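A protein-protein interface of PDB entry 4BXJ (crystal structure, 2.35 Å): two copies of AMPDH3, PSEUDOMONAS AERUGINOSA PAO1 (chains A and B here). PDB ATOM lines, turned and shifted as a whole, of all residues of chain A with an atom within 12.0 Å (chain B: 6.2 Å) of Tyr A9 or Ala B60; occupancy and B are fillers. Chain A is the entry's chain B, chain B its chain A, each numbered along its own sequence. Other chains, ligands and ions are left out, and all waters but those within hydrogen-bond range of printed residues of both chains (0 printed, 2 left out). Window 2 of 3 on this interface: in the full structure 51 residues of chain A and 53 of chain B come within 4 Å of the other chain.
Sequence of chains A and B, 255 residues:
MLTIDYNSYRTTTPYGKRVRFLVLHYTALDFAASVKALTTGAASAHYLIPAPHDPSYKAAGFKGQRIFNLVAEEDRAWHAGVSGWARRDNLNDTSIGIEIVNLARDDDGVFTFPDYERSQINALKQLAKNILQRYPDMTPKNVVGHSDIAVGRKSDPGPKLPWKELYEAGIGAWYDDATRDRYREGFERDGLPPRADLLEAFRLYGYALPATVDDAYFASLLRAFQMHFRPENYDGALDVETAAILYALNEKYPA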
ATOM      1  N   THR A   3      15.362  20.106   2.478  1.00  0.00           N
ATOM      2  CA  THR A   3      14.146  20.733   1.985  1.00  0.00           C
ATOM      3  C   THR A   3      13.526  19.779   0.969  1.00  0.00           C
ATOM      4  O   THR A   3      14.236  19.201   0.147  1.00  0.00           O
ATOM      5  CB  THR A   3      14.428  22.084   1.318  1.00  0.00           C
ATOM      6  OG1 THR A   3      15.194  22.907   2.197  1.00  0.00           O
ATOM      7  CG2 THR A   3      13.123  22.791   0.993  1.00  0.00           C
ATOM      8  N   ILE A   4      12.216  19.589   1.047  1.00  0.00           N
ATOM      9  CA  ILE A   4      11.538  18.659   0.158  1.00  0.00           C
ATOM     10  C   ILE A   4      11.608  19.175  -1.280  1.00  0.00           C
ATOM     11  O   ILE A   4      11.537  20.379  -1.506  1.00  0.00           O
ATOM     12  CB  ILE A   4      10.085  18.439   0.617  1.00  0.00           C
ATOM     13  CG1 ILE A   4      10.078  17.655   1.931  1.00  0.00           C
ATOM     14  CG2 ILE A   4       9.252  17.702  -0.459  1.00  0.00           C
ATOM     15  CD1 ILE A   4       8.717  17.576   2.600  1.00  0.00           C
ATOM     16  N   ASP A   5      11.791  18.278  -2.244  1.00  0.00           N
ATOM     17  CA  ASP A   5      11.882  18.677  -3.645  1.00  0.00           C
ATOM     18  C   ASP A   5      10.551  18.487  -4.357  1.00  0.00           C
ATOM     19  O   ASP A   5      10.122  17.353  -4.614  1.00  0.00           O
ATOM     20  CB  ASP A   5      12.949  17.854  -4.361  1.00  0.00           C
ATOM     21  CG  ASP A   5      13.231  18.350  -5.771  1.00  0.00           C
ATOM     22  OD1 ASP A   5      12.486  19.217  -6.276  1.00  0.00           O
ATOM     23  OD2 ASP A   5      14.201  17.858  -6.382  1.00  0.00           O
ATOM     24  N   TYR A   6       9.904  19.597  -4.701  1.00  0.00           N
ATOM     25  CA  TYR A   6       8.615  19.531  -5.390  1.00  0.00           C
ATOM     26  C   TYR A   6       8.722  19.824  -6.870  1.00  0.00           C
ATOM     27  O   TYR A   6       7.709  20.067  -7.504  1.00  0.00           O
ATOM     28  CB  TYR A   6       7.619  20.539  -4.812  1.00  0.00           C
ATOM     29  CG  TYR A   6       7.328  20.421  -3.342  1.00  0.00           C
ATOM     30  CD1 TYR A   6       8.084  21.125  -2.402  1.00  0.00           C
ATOM     31  CD2 TYR A   6       6.288  19.628  -2.886  1.00  0.00           C
ATOM     32  CE1 TYR A   6       7.804  21.026  -1.047  1.00  0.00           C
ATOM     33  CE2 TYR A   6       6.003  19.522  -1.539  1.00  0.00           C
ATOM     34  CZ  TYR A   6       6.763  20.224  -0.629  1.00  0.00           C
ATOM     35  OH  TYR A   6       6.481  20.124   0.705  1.00  0.00           O
ATOM     36  N   ASN A   7       9.922  19.829  -7.432  1.00  0.00           N
ATOM     37  CA  ASN A   7      10.056  20.289  -8.813  1.00  0.00           C
ATOM     38  C   ASN A   7      10.705  19.313  -9.753  1.00  0.00           C
ATOM     39  O   ASN A   7      10.495  19.391 -10.962  1.00  0.00           O
ATOM     40  CB  ASN A   7      10.849  21.588  -8.878  1.00  0.00           C
ATOM     41  CG  ASN A   7      10.050  22.781  -8.426  1.00  0.00           C
ATOM     42  OD1 ASN A   7      10.002  23.090  -7.239  1.00  0.00           O
ATOM     43  ND2 ASN A   7       9.441  23.480  -9.375  1.00  0.00           N
ATOM     44  N   SER A   8      11.528  18.420  -9.218  1.00  0.00           N
ATOM     45  CA  SER A   8      12.353  17.587 -10.082  1.00  0.00           C
ATOM     46  C   SER A   8      11.512  16.530 -10.772  1.00  0.00           C
ATOM     47  O   SER A   8      11.802  16.147 -11.902  1.00  0.00           O
ATOM     48  CB  SER A   8      13.513  16.956  -9.310  1.00  0.00           C
ATOM     49  OG  SER A   8      14.424  17.949  -8.859  1.00  0.00           O
ATOM     50  N   TYR A   9      10.466  16.065 -10.096  1.00  0.00           N
ATOM     51  CA  TYR A   9       9.578  15.071 -10.686  1.00  0.00           C
ATOM     52  C   TYR A   9       8.149  15.291 -10.238  1.00  0.00           C
ATOM     53  O   TYR A   9       7.902  15.639  -9.092  1.00  0.00           O
ATOM     54  CB  TYR A   9      10.024  13.661 -10.304  1.00  0.00           C
ATOM     55  CG  TYR A   9      11.460  13.366 -10.662  1.00  0.00           C
ATOM     56  CD1 TYR A   9      11.802  12.928 -11.926  1.00  0.00           C
ATOM     57  CD2 TYR A   9      12.478  13.538  -9.735  1.00  0.00           C
ATOM     58  CE1 TYR A   9      13.112  12.661 -12.261  1.00  0.00           C
ATOM     59  CE2 TYR A   9      13.792  13.273 -10.061  1.00  0.00           C
ATOM     60  CZ  TYR A   9      14.102  12.836 -11.324  1.00  0.00           C
ATOM     61  OH  TYR A   9      15.407  12.568 -11.651  1.00  0.00           O
ATOM     62  N   ARG A  10       7.203  15.078 -11.143  1.00  0.00           N
ATOM     63  CA  ARG A  10       5.792  15.199 -10.815  1.00  0.00           C
ATOM     64  C   ARG A  10       5.033  14.035 -11.416  1.00  0.00           C
ATOM     65  O   ARG A  10       5.241  13.678 -12.572  1.00  0.00           O
ATOM     66  CB  ARG A  10       5.239  16.493 -11.370  1.00  0.00           C
ATOM     67  CG  ARG A  10       5.950  17.738 -10.889  1.00  0.00           C
ATOM     68  CD  ARG A  10       5.189  18.379  -9.754  1.00  0.00           C
ATOM     69  NE  ARG A  10       5.512  17.744  -8.495  1.00  0.00           N
ATOM     70  CZ  ARG A  10       4.776  17.854  -7.393  1.00  0.00           C
ATOM     71  NH1 ARG A  10       3.656  18.573  -7.394  1.00  0.00           N
ATOM     72  NH2 ARG A  10       5.166  17.237  -6.282  1.00  0.00           N
ATOM     73  N   THR A  11       4.157  13.424 -10.634  1.00  0.00           N
ATOM     74  CA  THR A  11       3.367  12.320 -11.147  1.00  0.00           C
ATOM     75  C   THR A  11       2.328  12.873 -12.096  1.00  0.00           C
ATOM     76  O   THR A  11       1.741  13.912 -11.826  1.00  0.00           O
ATOM     77  CB  THR A  11       2.658  11.587 -10.027  1.00  0.00           C
ATOM     78  OG1 THR A  11       3.633  11.074  -9.126  1.00  0.00           O
ATOM     79  CG2 THR A  11       1.835  10.428 -10.580  1.00  0.00           C
ATOM     80  N   THR A  12       2.109  12.184 -13.208  1.00  0.00           N
ATOM     81  CA  THR A  12       1.117  12.611 -14.183  1.00  0.00           C
ATOM     82  C   THR A  12      -0.077  11.665 -14.199  1.00  0.00           C
ATOM     83  O   THR A  12      -1.116  11.968 -13.617  1.00  0.00           O
ATOM     84  CB  THR A  12       1.727  12.766 -15.579  1.00  0.00           C
ATOM     85  OG1 THR A  12       2.477  11.599 -15.903  1.00  0.00           O
ATOM     86  CG2 THR A  12       2.667  13.940 -15.605  1.00  0.00           C
ATOM     87  N   THR A  13       0.071  10.500 -14.817  1.00  0.00           N
ATOM     88  CA  THR A  13      -1.076   9.603 -14.938  1.00  0.00           C
ATOM     89  C   THR A  13      -1.562   8.922 -13.653  1.00  0.00           C
ATOM     90  O   THR A  13      -2.724   9.076 -13.294  1.00  0.00           O
ATOM     91  CB  THR A  13      -0.911   8.553 -16.065  1.00  0.00           C
ATOM     92  OG1 THR A  13       0.053   9.007 -17.026  1.00  0.00           O
ATOM     93  CG2 THR A  13      -2.236   8.351 -16.752  1.00  0.00           C
ATOM     94  N   PRO A  14      -0.691   8.164 -12.960  1.00  0.00           N
ATOM     95  CA  PRO A  14      -1.234   7.289 -11.912  1.00  0.00           C
ATOM     96  C   PRO A  14      -1.540   7.964 -10.582  1.00  0.00           C
ATOM     97  O   PRO A  14      -1.015   7.552  -9.558  1.00  0.00           O
ATOM     98  CB  PRO A  14      -0.113   6.269 -11.711  1.00  0.00           C
ATOM     99  CG  PRO A  14       1.117   7.047 -11.970  1.00  0.00           C
ATOM    100  CD  PRO A  14       0.769   7.989 -13.097  1.00  0.00           C
ATOM    101  N   TYR A  15      -2.393   8.975 -10.584  1.00  0.00           N
ATOM    102  CA  TYR A  15      -2.853   9.541  -9.325  1.00  0.00           C
ATOM    103  C   TYR A  15      -4.261  10.155  -9.468  1.00  0.00           C
ATOM    104  O   TYR A  15      -4.836  10.186 -10.563  1.00  0.00           O
ATOM    105  CB  TYR A  15      -1.820  10.542  -8.783  1.00  0.00           C
ATOM    106  CG  TYR A  15      -2.061  11.965  -9.197  1.00  0.00           C
ATOM    107  CD1 TYR A  15      -1.703  12.416 -10.459  1.00  0.00           C
ATOM    108  CD2 TYR A  15      -2.660  12.861  -8.328  1.00  0.00           C
ATOM    109  CE1 TYR A  15      -1.927  13.729 -10.838  1.00  0.00           C
ATOM    110  CE2 TYR A  15      -2.897  14.166  -8.698  1.00  0.00           C
ATOM    111  CZ  TYR A  15      -2.532  14.595  -9.955  1.00  0.00           C
ATOM    112  OH  TYR A  15      -2.774  15.902 -10.313  1.00  0.00           O
ATOM    113  N   PHE B  31      16.905   4.077  -8.773  1.00  0.00           N
ATOM    114  CA  PHE B  31      16.298   5.410  -8.831  1.00  0.00           C
ATOM    115  C   PHE B  31      15.643   5.721 -10.170  1.00  0.00           C
ATOM    116  O   PHE B  31      14.511   6.182 -10.218  1.00  0.00           O
ATOM    117  CB  PHE B  31      17.308   6.503  -8.512  1.00  0.00           C
ATOM    118  CG  PHE B  31      16.748   7.887  -8.630  1.00  0.00           C
ATOM    119  CD1 PHE B  31      16.103   8.478  -7.559  1.00  0.00           C
ATOM    120  CD2 PHE B  31      16.856   8.599  -9.816  1.00  0.00           C
ATOM    121  CE1 PHE B  31      15.591   9.750  -7.663  1.00  0.00           C
ATOM    122  CE2 PHE B  31      16.341   9.876  -9.925  1.00  0.00           C
ATOM    123  CZ  PHE B  31      15.713  10.450  -8.849  1.00  0.00           C
ATOM    124  N   VAL B  35      11.579   6.476 -10.390  1.00  0.00           N
ATOM    125  CA  VAL B  35      10.958   7.769 -10.656  1.00  0.00           C
ATOM    126  C   VAL B  35      10.110   7.665 -11.876  1.00  0.00           C
ATOM    127  O   VAL B  35       9.116   8.360 -12.002  1.00  0.00           O
ATOM    128  CB  VAL B  35      11.959   8.895 -10.873  1.00  0.00           C
ATOM    129  CG1 VAL B  35      12.640   9.208  -9.588  1.00  0.00           C
ATOM    130  CG2 VAL B  35      12.968   8.512 -11.944  1.00  0.00           C
ATOM    131  N   THR B  39       5.900   7.989 -11.564  1.00  0.00           N
ATOM    132  CA  THR B  39       5.398   9.234 -12.136  1.00  0.00           C
ATOM    133  C   THR B  39       4.561   9.012 -13.379  1.00  0.00           C
ATOM    134  O   THR B  39       3.592   9.744 -13.613  1.00  0.00           O
ATOM    135  CB  THR B  39       6.505  10.253 -12.462  1.00  0.00           C
ATOM    136  OG1 THR B  39       7.409   9.686 -13.411  1.00  0.00           O
ATOM    137  CG2 THR B  39       7.267  10.657 -11.200  1.00  0.00           C
ATOM    138  N   LEU B  48       9.296  10.102  -2.411  1.00  0.00           N
ATOM    139  CA  LEU B  48      10.316   9.131  -2.771  1.00  0.00           C
ATOM    140  C   LEU B  48      11.614   9.493  -2.076  1.00  0.00           C
ATOM    141  O   LEU B  48      12.067  10.641  -2.139  1.00  0.00           O
ATOM    142  CB  LEU B  48      10.542   9.143  -4.274  1.00  0.00           C
ATOM    143  CG  LEU B  48      11.628   8.227  -4.811  1.00  0.00           C
ATOM    144  CD1 LEU B  48      11.214   6.782  -4.688  1.00  0.00           C
ATOM    145  CD2 LEU B  48      11.880   8.570  -6.249  1.00  0.00           C
ATOM    146  N   PRO B  55      24.061   4.484  -9.025  1.00  0.00           N
ATOM    147  CA  PRO B  55      24.465   5.055 -10.317  1.00  0.00           C
ATOM    148  C   PRO B  55      23.300   5.733 -11.049  1.00  0.00           C
ATOM    149  O   PRO B  55      23.553   6.776 -11.652  1.00  0.00           O
ATOM    150  CB  PRO B  55      24.964   3.838 -11.093  1.00  0.00           C
ATOM    151  CG  PRO B  55      25.404   2.881 -10.027  1.00  0.00           C
ATOM    152  CD  PRO B  55      24.428   3.063  -8.908  1.00  0.00           C
ATOM    153  N   SER B  56      22.077   5.179 -10.981  1.00  0.00           N
ATOM    154  CA  SER B  56      20.887   5.822 -11.570  1.00  0.00           C
ATOM    155  C   SER B  56      20.745   7.217 -11.030  1.00  0.00           C
ATOM    156  O   SER B  56      20.436   8.158 -11.765  1.00  0.00           O
ATOM    157  CB  SER B  56      19.598   5.113 -11.171  1.00  0.00           C
ATOM    158  OG  SER B  56      19.510   3.832 -11.728  1.00  0.00           O
ATOM    159  N   TYR B  57      20.945   7.324  -9.720  1.00  0.00           N
ATOM    160  CA  TYR B  57      20.716   8.554  -8.999  1.00  0.00           C
ATOM    161  C   TYR B  57      21.737   9.594  -9.394  1.00  0.00           C
ATOM    162  O   TYR B  57      21.377  10.682  -9.843  1.00  0.00           O
ATOM    163  CB  TYR B  57      20.776   8.282  -7.502  1.00  0.00           C
ATOM    164  CG  TYR B  57      20.388   9.442  -6.610  1.00  0.00           C
ATOM    165  CD1 TYR B  57      19.145  10.051  -6.717  1.00  0.00           C
ATOM    166  CD2 TYR B  57      21.260   9.905  -5.639  1.00  0.00           C
ATOM    167  CE1 TYR B  57      18.799  11.097  -5.888  1.00  0.00           C
ATOM    168  CE2 TYR B  57      20.917  10.940  -4.812  1.00  0.00           C
ATOM    169  CZ  TYR B  57      19.682  11.527  -4.933  1.00  0.00           C
ATOM    170  OH  TYR B  57      19.353  12.560  -4.095  1.00  0.00           O
ATOM    171  N   LYS B  58      23.010   9.253  -9.228  1.00  0.00           N
ATOM    172  CA  LYS B  58      24.090  10.163  -9.572  1.00  0.00           C
ATOM    173  C   LYS B  58      23.966  10.563 -11.040  1.00  0.00           C
ATOM    174  O   LYS B  58      24.128  11.736 -11.389  1.00  0.00           O
ATOM    175  CB  LYS B  58      25.449   9.522  -9.283  1.00  0.00           C
ATOM    176  CG  LYS B  58      25.780   9.387  -7.792  1.00  0.00           C
ATOM    177  CD  LYS B  58      27.084   8.627  -7.607  1.00  0.00           C
ATOM    178  CE  LYS B  58      27.268   8.098  -6.193  1.00  0.00           C
ATOM    179  NZ  LYS B  58      28.463   7.183  -6.078  1.00  0.00           N
ATOM    180  N   ALA B  59      23.634   9.592 -11.890  1.00  0.00           N
ATOM    181  CA  ALA B  59      23.495   9.861 -13.321  1.00  0.00           C
ATOM    182  C   ALA B  59      22.369  10.843 -13.612  1.00  0.00           C
ATOM    183  O   ALA B  59      22.408  11.563 -14.599  1.00  0.00           O
ATOM    184  CB  ALA B  59      23.262   8.583 -14.077  1.00  0.00           C
ATOM    185  N   ALA B  60      21.360  10.868 -12.752  1.00  0.00           N
ATOM    186  CA  ALA B  60      20.224  11.744 -12.958  1.00  0.00           C
ATOM    187  C   ALA B  60      20.562  13.204 -12.647  1.00  0.00           C
ATOM    188  O   ALA B  60      19.792  14.106 -12.996  1.00  0.00           O
ATOM    189  CB  ALA B  60      19.054  11.275 -12.127  1.00  0.00           C
ATOM    190  N   GLY B  61      21.704  13.434 -11.991  1.00  0.00           N
ATOM    191  CA  GLY B  61      22.121  14.781 -11.627  1.00  0.00           C
ATOM    192  C   GLY B  61      22.401  14.982 -10.147  1.00  0.00           C
ATOM    193  O   GLY B  61      22.874  16.035  -9.725  1.00  0.00           O
ATOM    194  N   PHE B  62      22.126  13.962  -9.345  1.00  0.00           N
ATOM    195  CA  PHE B  62      22.137  14.140  -7.901  1.00  0.00           C
ATOM    196  C   PHE B  62      23.391  13.592  -7.212  1.00  0.00           C
ATOM    197  O   PHE B  62      24.167  12.851  -7.804  1.00  0.00           O
ATOM    198  CB  PHE B  62      20.868  13.536  -7.311  1.00  0.00           C
ATOM    199  CG  PHE B  62      19.620  14.033  -7.965  1.00  0.00           C
ATOM    200  CD1 PHE B  62      19.071  15.247  -7.600  1.00  0.00           C
ATOM    201  CD2 PHE B  62      19.009  13.301  -8.968  1.00  0.00           C
ATOM    202  CE1 PHE B  62      17.931  15.710  -8.211  1.00  0.00           C
ATOM    203  CE2 PHE B  62      17.866  13.763  -9.583  1.00  0.00           C
ATOM    204  CZ  PHE B  62      17.325  14.967  -9.205  1.00  0.00           C
ATOM    205  N   PHE B  68      11.960  13.664  -2.399  1.00  0.00           N
ATOM    206  CA  PHE B  68      11.150  14.108  -3.531  1.00  0.00           C
ATOM    207  C   PHE B  68       9.658  14.004  -3.250  1.00  0.00           C
ATOM    208  O   PHE B  68       9.172  12.957  -2.828  1.00  0.00           O
ATOM    209  CB  PHE B  68      11.442  13.276  -4.789  1.00  0.00           C
ATOM    210  CG  PHE B  68      12.827  13.436  -5.318  1.00  0.00           C
ATOM    211  CD1 PHE B  68      13.202  14.594  -5.968  1.00  0.00           C
ATOM    212  CD2 PHE B  68      13.752  12.410  -5.192  1.00  0.00           C
ATOM    213  CE1 PHE B  68      14.483  14.742  -6.459  1.00  0.00           C
ATOM    214  CE2 PHE B  68      15.033  12.546  -5.682  1.00  0.00           C
ATOM    215  CZ  PHE B  68      15.402  13.714  -6.314  1.00  0.00           C
ATOM    216  N   ASN B  69       8.927  15.081  -3.519  1.00  0.00           N
ATOM    217  CA  ASN B  69       7.480  15.003  -3.531  1.00  0.00           C
ATOM    218  C   ASN B  69       7.030  14.722  -4.951  1.00  0.00           C
ATOM    219  O   ASN B  69       7.486  15.362  -5.891  1.00  0.00           O
ATOM    220  CB  ASN B  69       6.859  16.286  -2.998  1.00  0.00           C
ATOM    221  CG  ASN B  69       5.334  16.236  -2.986  1.00  0.00           C
ATOM    222  OD1 ASN B  69       4.672  17.088  -3.573  1.00  0.00           O
ATOM    223  ND2 ASN B  69       4.774  15.228  -2.335  1.00  0.00           N
ATOM    224  N   LEU B  70       6.159  13.736  -5.108  1.00  0.00           N
ATOM    225  CA  LEU B  70       5.643  13.352  -6.423  1.00  0.00           C
ATOM    226  C   LEU B  70       4.155  13.670  -6.550  1.00  0.00           C
ATOM    227  O   LEU B  70       3.673  14.010  -7.629  1.00  0.00           O
ATOM    228  CB  LEU B  70       5.849  11.860  -6.668  1.00  0.00           C
ATOM    229  CG  LEU B  70       7.289  11.356  -6.687  1.00  0.00           C
ATOM    230  CD1 LEU B  70       7.323   9.950  -7.251  1.00  0.00           C
ATOM    231  CD2 LEU B  70       8.178  12.301  -7.477  1.00  0.00           C
ATOM    232  N   VAL B  71       3.439  13.523  -5.441  1.00  0.00           N
ATOM    233  CA  VAL B  71       2.018  13.818  -5.366  1.00  0.00           C
ATOM    234  C   VAL B  71       1.801  14.658  -4.119  1.00  0.00           C
ATOM    235  O   VAL B  71       2.340  14.337  -3.065  1.00  0.00           O
ATOM    236  CB  VAL B  71       1.171  12.534  -5.240  1.00  0.00           C
ATOM    237  CG1 VAL B  71      -0.303  12.865  -5.311  1.00  0.00           C
ATOM    238  CG2 VAL B  71       1.534  11.544  -6.324  1.00  0.00           C
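O of Thr B39 lies within hydrogen-bond range of N of Thr A12 (2.9 Å).
N of Asn B69 is in hydrogen-bond range of O of Asp A5, 2.8 Å away.
The side-chain amide oxygen (OD1) of Asn B69 lies within hydrogen-bond range of the guanidinium group (NH2) of Arg A10 (2.8 Å).
O of Leu B70 is in hydrogen-bond range of N of Thr A11 (3.1 Å).
The backbone carbonyl oxygen of Tyr A9 lies close to the backbone carbonyl oxygen of Asn B69 (3.2 Å).
OG1 of Thr B39 is in hydrogen-bond range of O of Val B35 (2.6 Å).
N of Leu B48 is in hydrogen-bond range of O of Phe B68 (2.9 Å).
O of Tyr B57 sits at hydrogen-bond distance from N of Phe B62 (3.4 Å).
The side-chain amide nitrogen (ND2) of Asn B69 sits at hydrogen-bond distance from the backbone carbonyl oxygen (O) of Val B71 (2.7 Å).
The side-chain carboxylate (OD1) of Asp A5 sits at hydrogen-bond distance from the backbone NH (N) of Asn A7 (2.9 Å).
The side-chain carboxylate of Asp A5 sits at hydrogen-bond distance from the side-chain hydroxyl of Ser A8 (2.5 Å).
Among the printed residues, merely in contact across the chains: Ile A4 with Asn B69 (3.8 Å), Asp A5 with Phe B68 (3.1 Å), Tyr A6 with Asn B69 (3.1 Å), Ser A8 with Phe B68 (3.7 Å), Tyr A9 with Phe B31 (3.3 Å), Tyr A9 with Ala B60 (3.9 Å), Tyr A9 with Phe B62 (3.4 Å), Tyr A9 with Phe B68 (3.95 Å), Tyr A9 with Leu B70 (3.6 Å), Arg A10 with Thr B39 (3.7 Å), Arg A10 with Leu B70 (3.7 Å), Thr A11 with Thr B39 (3.6 Å), Thr A11 with Val B71 (3.5 Å), Thr A13 with Thr B39 (3.8 Å), Pro A14 with Thr B39 (3.4 Å) and Tyr A15 with Val B71 (3.8 Å).
Tyr A9 touches six residues of chain B.
Ala B60 touches just one residue of chain A: Tyr A9 (3.9 Å).
No residue of chain A comes within 4 Å of Val B35.
Of the printed residues of chain A, Thr B39 touches Arg A10 (3.7 Å), Thr A11 (3.6 Å), Thr A12 (2.9 Å), Thr A13 (3.8 Å) and Pro A14 (3.4 Å).
Ser B56 touches none of the printed residues of chain A.
No residue of chain A comes within 4 Å of Ala B59.
No residue of chain A comes within 4 Å of Gly B61.
Phe B62 touches just one residue of chain A: Tyr A9.
Phe B68 touches just these residues of chain A: Asp A5, Ser A8 and Tyr A9.
Of the printed residues of chain A, Asn B69 touches Ile A4, Asp A5, Tyr A6, Tyr A9 and Arg A10.
Leu B70 touches just these residues of chain A: Tyr A9, Arg A10 and Thr A11.
Of the printed residues of chain B, Tyr A6 touches Asn B69.
Printed residues of chain B within 4 Å of Pro A14: Thr B39.
Of the printed residues of chain A, Val B71 touches Thr A11 (3.5 Å) and Tyr A15 (3.8 Å).
Asn A7 touches none of the printed residues of chain B.
The nearest printed residue of chain B that does not touch Tyr A9 is Val B35 (4.2 Å).
The nearest residue of chain A that does not touch Ala B60 is Ser A8 (7.8 Å).
Along chain B the printed residues that touch a printed residue of chain A span positions 31 to 71.
Among the printed residues, 21 pairs touch across the chains.
Among the printed residues, no Asp or Glu carboxylate lies within 4 Å of a Lys or Arg side-chain nitrogen of the other chain.
No position is printed for both chains.
Of the 21 pairs that touch across the chains among the printed residues, none has its exchanged pair printed and touching as well.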
